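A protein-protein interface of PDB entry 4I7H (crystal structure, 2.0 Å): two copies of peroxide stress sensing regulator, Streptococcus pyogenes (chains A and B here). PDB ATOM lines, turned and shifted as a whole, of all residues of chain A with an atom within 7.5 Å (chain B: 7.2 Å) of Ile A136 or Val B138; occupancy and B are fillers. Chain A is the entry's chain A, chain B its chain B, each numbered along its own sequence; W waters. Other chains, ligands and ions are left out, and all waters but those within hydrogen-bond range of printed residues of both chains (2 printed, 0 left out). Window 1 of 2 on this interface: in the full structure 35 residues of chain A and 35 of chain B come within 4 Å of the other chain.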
ATOM      1  N   ASP A  11      23.399  32.202 -12.310  1.00  0.00           N
ATOM      2  CA  ASP A  11      22.089  32.267 -11.646  1.00  0.00           C
ATOM      3  C   ASP A  11      21.117  33.055 -12.527  1.00  0.00           C
ATOM      4  O   ASP A  11      21.486  33.479 -13.637  1.00  0.00           O
ATOM      5  CB  ASP A  11      22.174  32.818 -10.214  1.00  0.00           C
ATOM      6  CG  ASP A  11      22.660  34.265 -10.154  1.00  0.00           C
ATOM      7  OD1 ASP A  11      22.630  34.982 -11.181  1.00  0.00           O
ATOM      8  OD2 ASP A  11      23.046  34.702  -9.048  1.00  0.00           O
ATOM      9  N   GLN A  98      17.932  29.487 -15.282  1.00  0.00           N
ATOM     10  CA  GLN A  98      19.344  29.615 -14.910  1.00  0.00           C
ATOM     11  C   GLN A  98      20.158  28.412 -15.355  1.00  0.00           C
ATOM     12  O   GLN A  98      19.629  27.483 -15.978  1.00  0.00           O
ATOM     13  CB  GLN A  98      19.523  29.832 -13.410  1.00  0.00           C
ATOM     14  CG  GLN A  98      19.163  28.641 -12.557  1.00  0.00           C
ATOM     15  CD  GLN A  98      19.135  29.026 -11.094  1.00  0.00           C
ATOM     16  OE1 GLN A  98      18.071  29.320 -10.541  1.00  0.00           O
ATOM     17  NE2 GLN A  98      20.305  29.076 -10.468  1.00  0.00           N
ATOM     18  N   ASP A 117      13.529  25.107 -12.270  1.00  0.00           N
ATOM     19  CA  ASP A 117      12.900  24.664 -11.023  1.00  0.00           C
ATOM     20  C   ASP A 117      13.407  25.311  -9.724  1.00  0.00           C
ATOM     21  O   ASP A 117      12.645  25.402  -8.752  1.00  0.00           O
ATOM     22  CB  ASP A 117      12.977  23.144 -10.906  1.00  0.00           C
ATOM     23  CG  ASP A 117      12.199  22.438 -12.002  1.00  0.00           C
ATOM     24  OD1 ASP A 117      11.090  22.893 -12.349  1.00  0.00           O
ATOM     25  OD2 ASP A 117      12.713  21.432 -12.522  1.00  0.00           O
ATOM     26  N   VAL A 118      14.667  25.757  -9.686  1.00  0.00           N
ATOM     27  CA  VAL A 118      15.176  26.407  -8.468  1.00  0.00           C
ATOM     28  C   VAL A 118      14.306  27.595  -8.066  1.00  0.00           C
ATOM     29  O   VAL A 118      14.058  27.818  -6.870  1.00  0.00           O
ATOM     30  CB  VAL A 118      16.661  26.837  -8.567  1.00  0.00           C
ATOM     31  CG1 VAL A 118      17.077  27.583  -7.296  1.00  0.00           C
ATOM     32  CG2 VAL A 118      17.554  25.629  -8.768  1.00  0.00           C
ATOM     33  N   MET A 119      13.817  28.340  -9.055  1.00  0.00           N
ATOM     34  CA  MET A 119      12.892  29.436  -8.762  1.00  0.00           C
ATOM     35  C   MET A 119      11.619  28.942  -8.053  1.00  0.00           C
ATOM     36  O   MET A 119      11.064  29.639  -7.208  1.00  0.00           O
ATOM     37  CB  MET A 119      12.522  30.213 -10.038  1.00  0.00           C
ATOM     38  CG  MET A 119      13.596  31.195 -10.513  1.00  0.00           C
ATOM     39  SD  MET A 119      14.033  32.483  -9.304  1.00  0.00           S
ATOM     40  CE  MET A 119      12.701  33.689  -9.520  1.00  0.00           C
ATOM     41  N   ASP A 120      11.158  27.744  -8.398  1.00  0.00           N
ATOM     42  CA  ASP A 120       9.976  27.192  -7.739  1.00  0.00           C
ATOM     43  C   ASP A 120      10.284  26.809  -6.289  1.00  0.00           C
ATOM     44  O   ASP A 120       9.430  26.952  -5.412  1.00  0.00           O
ATOM     45  CB  ASP A 120       9.399  26.004  -8.520  1.00  0.00           C
ATOM     46  CG  ASP A 120       8.610  26.440  -9.755  1.00  0.00           C
ATOM     47  OD1 ASP A 120       8.172  27.610  -9.798  1.00  0.00           O
ATOM     48  OD2 ASP A 120       8.418  25.615 -10.681  1.00  0.00           O
ATOM     49  N   ILE A 121      11.505  26.347  -6.039  1.00  0.00           N
ATOM     50  CA  ILE A 121      11.938  26.068  -4.672  1.00  0.00           C
ATOM     51  C   ILE A 121      11.888  27.345  -3.826  1.00  0.00           C
ATOM     52  O   ILE A 121      11.376  27.345  -2.708  1.00  0.00           O
ATOM     53  CB  ILE A 121      13.354  25.473  -4.637  1.00  0.00           C
ATOM     54  CG1 ILE A 121      13.376  24.145  -5.397  1.00  0.00           C
ATOM     55  CG2 ILE A 121      13.810  25.274  -3.183  1.00  0.00           C
ATOM     56  CD1 ILE A 121      14.774  23.582  -5.610  1.00  0.00           C
ATOM     57  N   ALA A 122      12.404  28.438  -4.377  1.00  0.00           N
ATOM     58  CA  ALA A 122      12.380  29.734  -3.704  1.00  0.00           C
ATOM     59  C   ALA A 122      10.945  30.128  -3.351  1.00  0.00           C
ATOM     60  O   ALA A 122      10.664  30.627  -2.252  1.00  0.00           O
ATOM     61  CB  ALA A 122      13.013  30.805  -4.601  1.00  0.00           C
ATOM     62  N   LYS A 123      10.039  29.899  -4.292  1.00  0.00           N
ATOM     63  CA  LYS A 123       8.636  30.255  -4.094  1.00  0.00           C
ATOM     64  C   LYS A 123       7.997  29.404  -2.990  1.00  0.00           C
ATOM     65  O   LYS A 123       7.306  29.933  -2.116  1.00  0.00           O
ATOM     66  CB  LYS A 123       7.862  30.134  -5.411  1.00  0.00           C
ATOM     67  CG  LYS A 123       6.381  30.361  -5.280  1.00  0.00           C
ATOM     68  CD  LYS A 123       5.784  31.030  -6.521  1.00  0.00           C
ATOM     69  CE  LYS A 123       5.677  30.075  -7.710  1.00  0.00           C
ATOM     70  NZ  LYS A 123       4.500  30.414  -8.583  1.00  0.00           N
ATOM     71  N   ALA A 125       9.559  27.872  -0.529  1.00  0.00           N
ATOM     72  CA  ALA A 125      10.168  28.317   0.716  1.00  0.00           C
ATOM     73  C   ALA A 125       9.462  29.567   1.231  1.00  0.00           C
ATOM     74  O   ALA A 125       9.103  29.632   2.407  1.00  0.00           O
ATOM     75  CB  ALA A 125      11.674  28.571   0.544  1.00  0.00           C
ATOM     76  N   VAL A 133      13.521  34.812   0.290  1.00  0.00           N
ATOM     77  CA  VAL A 133      14.654  34.025  -0.188  1.00  0.00           C
ATOM     78  C   VAL A 133      15.648  34.897  -0.938  1.00  0.00           C
ATOM     79  O   VAL A 133      15.275  35.647  -1.842  1.00  0.00           O
ATOM     80  CB  VAL A 133      14.184  32.878  -1.083  1.00  0.00           C
ATOM     81  CG1 VAL A 133      15.380  32.108  -1.660  1.00  0.00           C
ATOM     82  CG2 VAL A 133      13.267  31.961  -0.290  1.00  0.00           C
ATOM     83  N   THR A 134      16.915  34.798  -0.553  1.00  0.00           N
ATOM     84  CA  THR A 134      17.957  35.607  -1.171  1.00  0.00           C
ATOM     85  C   THR A 134      18.765  34.793  -2.170  1.00  0.00           C
ATOM     86  O   THR A 134      19.164  35.300  -3.222  1.00  0.00           O
ATOM     87  CB  THR A 134      18.905  36.181  -0.120  1.00  0.00           C
ATOM     88  OG1 THR A 134      19.318  35.133   0.766  1.00  0.00           O
ATOM     89  CG2 THR A 134      18.203  37.252   0.688  1.00  0.00           C
ATOM     90  N   ARG A 135      19.003  33.527  -1.851  1.00  0.00           N
ATOM     91  CA  ARG A 135      19.775  32.676  -2.754  1.00  0.00           C
ATOM     92  C   ARG A 135      19.629  31.200  -2.419  1.00  0.00           C
ATOM     93  O   ARG A 135      19.500  30.822  -1.245  1.00  0.00           O
ATOM     94  CB  ARG A 135      21.252  33.052  -2.677  1.00  0.00           C
ATOM     95  CG  ARG A 135      21.785  33.045  -1.261  1.00  0.00           C
ATOM     96  CD  ARG A 135      23.253  33.449  -1.193  1.00  0.00           C
ATOM     97  NE  ARG A 135      23.745  33.288   0.174  1.00  0.00           N
ATOM     98  CZ  ARG A 135      24.543  32.306   0.572  1.00  0.00           C
ATOM     99  NH1 ARG A 135      24.983  31.401  -0.303  1.00  0.00           N
ATOM    100  NH2 ARG A 135      24.913  32.239   1.846  1.00  0.00           N
ATOM    101  N   ILE A 136      19.666  30.366  -3.455  1.00  0.00           N
ATOM    102  CA  ILE A 136      19.706  28.921  -3.272  1.00  0.00           C
ATOM    103  C   ILE A 136      20.827  28.356  -4.139  1.00  0.00           C
ATOM    104  O   ILE A 136      20.615  28.027  -5.313  1.00  0.00           O
ATOM    105  CB  ILE A 136      18.367  28.242  -3.631  1.00  0.00           C
ATOM    106  CG1 ILE A 136      17.195  28.949  -2.934  1.00  0.00           C
ATOM    107  CG2 ILE A 136      18.393  26.750  -3.259  1.00  0.00           C
ATOM    108  CD1 ILE A 136      15.839  28.361  -3.290  1.00  0.00           C
ATOM    109  N   PRO A 137      22.032  28.244  -3.558  1.00  0.00           N
ATOM    110  CA  PRO A 137      23.170  27.663  -4.270  1.00  0.00           C
ATOM    111  C   PRO A 137      22.833  26.212  -4.578  1.00  0.00           C
ATOM    112  O   PRO A 137      22.473  25.456  -3.675  1.00  0.00           O
ATOM    113  CB  PRO A 137      24.310  27.743  -3.249  1.00  0.00           C
ATOM    114  CG  PRO A 137      23.627  27.767  -1.908  1.00  0.00           C
ATOM    115  CD  PRO A 137      22.316  28.476  -2.126  1.00  0.00           C
ATOM    116  N   VAL A 138      22.875  25.841  -5.850  1.00  0.00           N
ATOM    117  CA  VAL A 138      22.609  24.457  -6.215  1.00  0.00           C
ATOM    118  C   VAL A 138      23.733  23.901  -7.083  1.00  0.00           C
ATOM    119  O   VAL A 138      24.091  24.484  -8.104  1.00  0.00           O
ATOM    120  CB  VAL A 138      21.263  24.307  -6.952  1.00  0.00           C
ATOM    121  CG1 VAL A 138      21.053  22.854  -7.351  1.00  0.00           C
ATOM    122  CG2 VAL A 138      20.096  24.812  -6.083  1.00  0.00           C
ATOM    123  N   ILE A 139      24.311  22.784  -6.655  1.00  0.00           N
ATOM    124  CA  ILE A 139      25.259  22.061  -7.490  1.00  0.00           C
ATOM    125  C   ILE A 139      24.827  20.597  -7.507  1.00  0.00           C
ATOM    126  O   ILE A 139      24.547  20.026  -6.456  1.00  0.00           O
ATOM    127  CB  ILE A 139      26.699  22.189  -6.953  1.00  0.00           C
ATOM    128  CG1 ILE A 139      27.138  23.655  -6.959  1.00  0.00           C
ATOM    129  CG2 ILE A 139      27.657  21.342  -7.772  1.00  0.00           C
ATOM    130  CD1 ILE A 139      28.375  23.921  -6.127  1.00  0.00           C
ATOM    131  N   ALA B   9      15.104  18.947   8.275  1.00  0.00           N
ATOM    132  CA  ALA B   9      15.294  18.547   6.886  1.00  0.00           C
ATOM    133  C   ALA B   9      15.298  17.016   6.822  1.00  0.00           C
ATOM    134  O   ALA B   9      15.787  16.340   7.731  1.00  0.00           O
ATOM    135  CB  ALA B   9      16.602  19.117   6.328  1.00  0.00           C
ATOM    136  N   GLN B  98      10.369  15.963  -0.156  1.00  0.00           N
ATOM    137  CA  GLN B  98      11.400  15.979   0.864  1.00  0.00           C
ATOM    138  C   GLN B  98      11.228  17.265   1.675  1.00  0.00           C
ATOM    139  O   GLN B  98      10.312  18.054   1.415  1.00  0.00           O
ATOM    140  CB  GLN B  98      12.803  15.914   0.233  1.00  0.00           C
ATOM    141  CG  GLN B  98      13.167  17.153  -0.613  1.00  0.00           C
ATOM    142  CD  GLN B  98      14.655  17.213  -1.009  1.00  0.00           C
ATOM    143  OE1 GLN B  98      15.488  16.469  -0.488  1.00  0.00           O
ATOM    144  NE2 GLN B  98      14.985  18.126  -1.921  1.00  0.00           N
ATOM    145  N   HIS B  99      12.103  17.472   2.651  1.00  0.00           N
ATOM    146  CA  HIS B  99      12.046  18.669   3.491  1.00  0.00           C
ATOM    147  C   HIS B  99      13.408  19.299   3.548  1.00  0.00           C
ATOM    148  O   HIS B  99      14.394  18.614   3.825  1.00  0.00           O
ATOM    149  CB  HIS B  99      11.562  18.315   4.895  1.00  0.00           C
ATOM    150  CG  HIS B  99      10.130  17.906   4.925  1.00  0.00           C
ATOM    151  ND1 HIS B  99       9.112  18.828   5.030  1.00  0.00           N
ATOM    152  CD2 HIS B  99       9.536  16.694   4.788  1.00  0.00           C
ATOM    153  CE1 HIS B  99       7.951  18.202   5.006  1.00  0.00           C
ATOM    154  NE2 HIS B  99       8.180  16.917   4.844  1.00  0.00           N
ATOM    155  N   VAL B 100      13.461  20.598   3.255  1.00  0.00           N
ATOM    156  CA  VAL B 100      14.736  21.299   3.198  1.00  0.00           C
ATOM    157  C   VAL B 100      14.760  22.565   4.060  1.00  0.00           C
ATOM    158  O   VAL B 100      13.704  23.148   4.368  1.00  0.00           O
ATOM    159  CB  VAL B 100      15.208  21.531   1.718  1.00  0.00           C
ATOM    160  CG1 VAL B 100      14.191  21.028   0.721  1.00  0.00           C
ATOM    161  CG2 VAL B 100      15.594  22.988   1.440  1.00  0.00           C
ATOM    162  N   ASN B 101      15.957  22.963   4.472  1.00  0.00           N
ATOM    163  CA  ASN B 101      16.115  24.120   5.354  1.00  0.00           C
ATOM    164  C   ASN B 101      16.235  25.450   4.623  1.00  0.00           C
ATOM    165  O   ASN B 101      16.745  25.491   3.500  1.00  0.00           O
ATOM    166  CB  ASN B 101      17.332  23.900   6.258  1.00  0.00           C
ATOM    167  CG  ASN B 101      17.069  22.862   7.329  1.00  0.00           C
ATOM    168  OD1 ASN B 101      15.976  22.822   7.902  1.00  0.00           O
ATOM    169  ND2 ASN B 101      18.057  22.023   7.611  1.00  0.00           N
ATOM    170  N   VAL B 102      15.736  26.525   5.247  1.00  0.00           N
ATOM    171  CA  VAL B 102      16.113  27.895   4.861  1.00  0.00           C
ATOM    172  C   VAL B 102      16.792  28.539   6.068  1.00  0.00           C
ATOM    173  O   VAL B 102      16.298  28.414   7.191  1.00  0.00           O
ATOM    174  CB  VAL B 102      14.920  28.820   4.575  1.00  0.00           C
ATOM    175  CG1 VAL B 102      15.319  29.922   3.575  1.00  0.00           C
ATOM    176  CG2 VAL B 102      13.716  28.057   4.127  1.00  0.00           C
ATOM    177  N   PHE B 113      10.937  23.561   4.990  1.00  0.00           N
ATOM    178  CA  PHE B 113       9.802  23.583   4.097  1.00  0.00           C
ATOM    179  C   PHE B 113       9.788  22.320   3.239  1.00  0.00           C
ATOM    180  O   PHE B 113      10.803  21.621   3.084  1.00  0.00           O
ATOM    181  CB  PHE B 113       9.792  24.858   3.248  1.00  0.00           C
ATOM    182  CG  PHE B 113      10.920  24.939   2.252  1.00  0.00           C
ATOM    183  CD1 PHE B 113      10.725  24.539   0.929  1.00  0.00           C
ATOM    184  CD2 PHE B 113      12.170  25.415   2.629  1.00  0.00           C
ATOM    185  CE1 PHE B 113      11.760  24.610   0.005  1.00  0.00           C
ATOM    186  CE2 PHE B 113      13.219  25.481   1.700  1.00  0.00           C
ATOM    187  CZ  PHE B 113      13.000  25.081   0.392  1.00  0.00           C
ATOM    188  N   ASP B 115       9.451  20.223  -0.133  1.00  0.00           N
ATOM    189  CA  ASP B 115       9.892  20.447  -1.510  1.00  0.00           C
ATOM    190  C   ASP B 115       9.552  19.265  -2.403  1.00  0.00           C
ATOM    191  O   ASP B 115       9.675  18.118  -1.984  1.00  0.00           O
ATOM    192  CB  ASP B 115      11.400  20.640  -1.557  1.00  0.00           C
ATOM    193  CG  ASP B 115      11.964  20.465  -2.973  1.00  0.00           C
ATOM    194  OD1 ASP B 115      11.754  21.371  -3.831  1.00  0.00           O
ATOM    195  OD2 ASP B 115      12.599  19.417  -3.230  1.00  0.00           O
ATOM    196  N   VAL B 118      13.157  19.445  -6.360  1.00  0.00           N
ATOM    197  CA  VAL B 118      14.538  19.000  -6.551  1.00  0.00           C
ATOM    198  C   VAL B 118      14.597  17.742  -7.436  1.00  0.00           C
ATOM    199  O   VAL B 118      15.516  17.587  -8.245  1.00  0.00           O
ATOM    200  CB  VAL B 118      15.320  18.852  -5.218  1.00  0.00           C
ATOM    201  CG1 VAL B 118      16.683  18.211  -5.454  1.00  0.00           C
ATOM    202  CG2 VAL B 118      15.497  20.218  -4.556  1.00  0.00           C
ATOM    203  N   ILE B 121      14.928  18.498 -11.003  1.00  0.00           N
ATOM    204  CA  ILE B 121      16.237  19.045 -11.339  1.00  0.00           C
ATOM    205  C   ILE B 121      17.168  17.897 -11.672  1.00  0.00           C
ATOM    206  O   ILE B 121      17.935  17.974 -12.629  1.00  0.00           O
ATOM    207  CB  ILE B 121      16.827  19.894 -10.190  1.00  0.00           C
ATOM    208  CG1 ILE B 121      15.901  21.067  -9.876  1.00  0.00           C
ATOM    209  CG2 ILE B 121      18.229  20.391 -10.533  1.00  0.00           C
ATOM    210  CD1 ILE B 121      16.419  21.986  -8.754  1.00  0.00           C
ATOM    211  N   ILE B 136      21.859  15.924  -5.150  1.00  0.00           N
ATOM    212  CA  ILE B 136      21.722  17.365  -5.328  1.00  0.00           C
ATOM    213  C   ILE B 136      21.379  17.990  -3.971  1.00  0.00           C
ATOM    214  O   ILE B 136      20.210  18.236  -3.675  1.00  0.00           O
ATOM    215  CB  ILE B 136      20.625  17.728  -6.338  1.00  0.00           C
ATOM    216  CG1 ILE B 136      20.876  17.027  -7.678  1.00  0.00           C
ATOM    217  CG2 ILE B 136      20.570  19.240  -6.552  1.00  0.00           C
ATOM    218  CD1 ILE B 136      19.892  17.402  -8.737  1.00  0.00           C
ATOM    219  N   PRO B 137      22.399  18.214  -3.133  1.00  0.00           N
ATOM    220  CA  PRO B 137      22.188  18.752  -1.776  1.00  0.00           C
ATOM    221  C   PRO B 137      21.781  20.227  -1.823  1.00  0.00           C
ATOM    222  O   PRO B 137      22.458  21.031  -2.446  1.00  0.00           O
ATOM    223  CB  PRO B 137      23.561  18.589  -1.114  1.00  0.00           C
ATOM    224  CG  PRO B 137      24.538  18.528  -2.246  1.00  0.00           C
ATOM    225  CD  PRO B 137      23.820  17.938  -3.419  1.00  0.00           C
ATOM    226  N   VAL B 138      20.679  20.567  -1.166  1.00  0.00           N
ATOM    227  CA  VAL B 138      20.108  21.902  -1.256  1.00  0.00           C
ATOM    228  C   VAL B 138      19.802  22.495   0.115  1.00  0.00           C
ATOM    229  O   VAL B 138      19.315  21.796   1.012  1.00  0.00           O
ATOM    230  CB  VAL B 138      18.823  21.895  -2.124  1.00  0.00           C
ATOM    231  CG1 VAL B 138      18.152  23.277  -2.157  1.00  0.00           C
ATOM    232  CG2 VAL B 138      19.166  21.447  -3.568  1.00  0.00           C
ATOM    233  N   ILE B 139      20.126  23.778   0.268  1.00  0.00           N
ATOM    234  CA  ILE B 139      19.722  24.576   1.426  1.00  0.00           C
ATOM    235  C   ILE B 139      19.423  25.972   0.889  1.00  0.00           C
ATOM    236  O   ILE B 139      20.112  26.458  -0.003  1.00  0.00           O
ATOM    237  CB  ILE B 139      20.842  24.655   2.491  1.00  0.00           C
ATOM    238  CG1 ILE B 139      20.362  25.387   3.744  1.00  0.00           C
ATOM    239  CG2 ILE B 139      22.102  25.323   1.920  1.00  0.00           C
ATOM    240  CD1 ILE B 139      21.197  25.049   4.978  1.00  0.00           C
ATOM    241  N   ALA B 140      18.381  26.605   1.406  1.00  0.00           N
ATOM    242  CA  ALA B 140      18.025  27.927   0.946  1.00  0.00           C
ATOM    243  C   ALA B 140      18.490  28.976   1.962  1.00  0.00           C
ATOM    244  O   ALA B 140      18.607  28.698   3.164  1.00  0.00           O
ATOM    245  CB  ALA B 140      16.538  28.021   0.718  1.00  0.00           C
ATOM    246  N   TYR B 141      18.770  30.173   1.467  1.00  0.00           N
ATOM    247  CA  TYR B 141      19.129  31.284   2.333  1.00  0.00           C
ATOM    248  C   TYR B 141      18.136  32.407   2.121  1.00  0.00           C
ATOM    249  O   TYR B 141      17.706  32.666   0.983  1.00  0.00           O
ATOM    250  CB  TYR B 141      20.549  31.772   2.059  1.00  0.00           C
ATOM    251  CG  TYR B 141      21.591  30.783   2.485  1.00  0.00           C
ATOM    252  CD1 TYR B 141      22.101  29.858   1.585  1.00  0.00           C
ATOM    253  CD2 TYR B 141      22.044  30.744   3.802  1.00  0.00           C
ATOM    254  CE1 TYR B 141      23.049  28.929   1.977  1.00  0.00           C
ATOM    255  CE2 TYR B 141      22.990  29.827   4.202  1.00  0.00           C
ATOM    256  CZ  TYR B 141      23.492  28.922   3.285  1.00  0.00           C
ATOM    257  OH  TYR B 141      24.438  28.007   3.680  1.00  0.00           O
HETATM  258  O   HOH W   1      26.647  29.561   2.908  1.00  0.00           O
HETATM  259  O   HOH W   2      24.496  21.406  -4.132  1.00  0.00           O
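CB of Asp A117 touches CG1 of Ile B121 (3.7 Å). Phe B113 touches Ile A121. Asp B115 touches Ile A121. Val B118 touches Ile A121. Tyr B141 touches Val A133. Ile A136 touches Val B138 (CG2 to CG1, 3.7 Å). O of Ile B139 touches CG2 of Ile A136, at 3.7 Å. Ile B139 touches Pro A137. Pro A137 touches Tyr B141 (CD to CD1, 3.97 Å). CG2 of Ile B136 touches CG1 of Val A138, at 3.7 Å.
Hydrophobic or aromatic side chains of chain B that line the printed part of chain A: Phe B113, Val B118, Ile B121, Ile B136, Pro B137, Val B138, Ala B140 and Tyr B141. Of the 17 printed residues of chain A, 11 touch a printed residue of chain B. Hydrophobic or aromatic side chains of chain A that line the printed part of chain B: Val A118, Ile A121, Ala A125, Val A133, Ile A136, Pro A137 and Val A138. Along chain A the printed residues that touch a printed residue of chain B span positions 117 to 139. Among the printed residues, 18 pairs touch across the chains.
Water W2 lies within hydrogen-bond range of the backbone carbonyl oxygen (O) of Pro B137 (2.7 Å) and the backbone carbonyl oxygen (O) of Ile A139 (2.7 Å). Water W1 lies within hydrogen-bond range of the side-chain hydroxyl (OH) of Tyr B141 (2.8 Å) and the guanidinium group (NH2) of Arg A135 (3.4 Å).
N of Thr A134 lies within hydrogen-bond range of O of Tyr B141 (2.7 Å). The backbone NH (N) of Tyr B141 lies within hydrogen-bond range of the backbone carbonyl oxygen (O) of Arg A135 (2.9 Å).
The backbone carbonyl oxygen (O) of Gln B98 is in hydrogen-bond range of the backbone NH (N) of Asp B115 (2.8 Å). The backbone NH (N) of Val B100 is in hydrogen-bond range of the backbone carbonyl oxygen (O) of Phe B113, 2.9 Å away. The backbone NH (N) of Ala B140 sits at hydrogen-bond distance from the backbone carbonyl oxygen (O) of Asn B101 (2.9 Å). The backbone NH of Val B118 is in hydrogen-bond range of the side-chain carboxylate of Asp B115.
Val A118 touches Ile B121, and with the chains exchanged Ile A121 touches Val B118. Ile A121 touches its own counterpart, Ile B121. Ile A136 touches Val B138, and with the chains exchanged Val A138 touches Ile B136. Ile A136 touches Ile B139, but with the chains exchanged Ile A139 does not touch Ile B136 (4.04 Å). Positions printed for both chains: 98, 118, 121, 136, 137, 138 and 139. Of the 18 pairs that touch across the chains among the printed residues, 7 have their exchanged pair printed and touching as well.
Ile A136 touches just these residues of chain B: Val B138 (3.7 Å), Ile B139 (3.7 Å) and Ala B140 (3.8 Å). Of chain A, only Ile A136 (3.7 Å) comes within 4 Å of Val B138. Of the printed residues of chain B, Ala A125 touches Phe B113 (3.6 Å). Of the printed residues of chain B, Val A138 touches Ile B136 (3.7 Å). Of the printed residues of chain A, Ala B140 touches Arg A135 and Ile A136. Printed residues of chain B within 4 Å of Thr A134: Tyr B141 (2.7 Å). Of the printed residues of chain A, Asp B115 touches Ile A121 (3.6 Å). Asp A11 touches none of the printed residues of chain B. The nearest residue of chain B that does not touch Ile A136 is Tyr B141 (4.8 Å). The nearest residue of chain A that does not touch Val B138 is Val A138 (4.3 Å).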
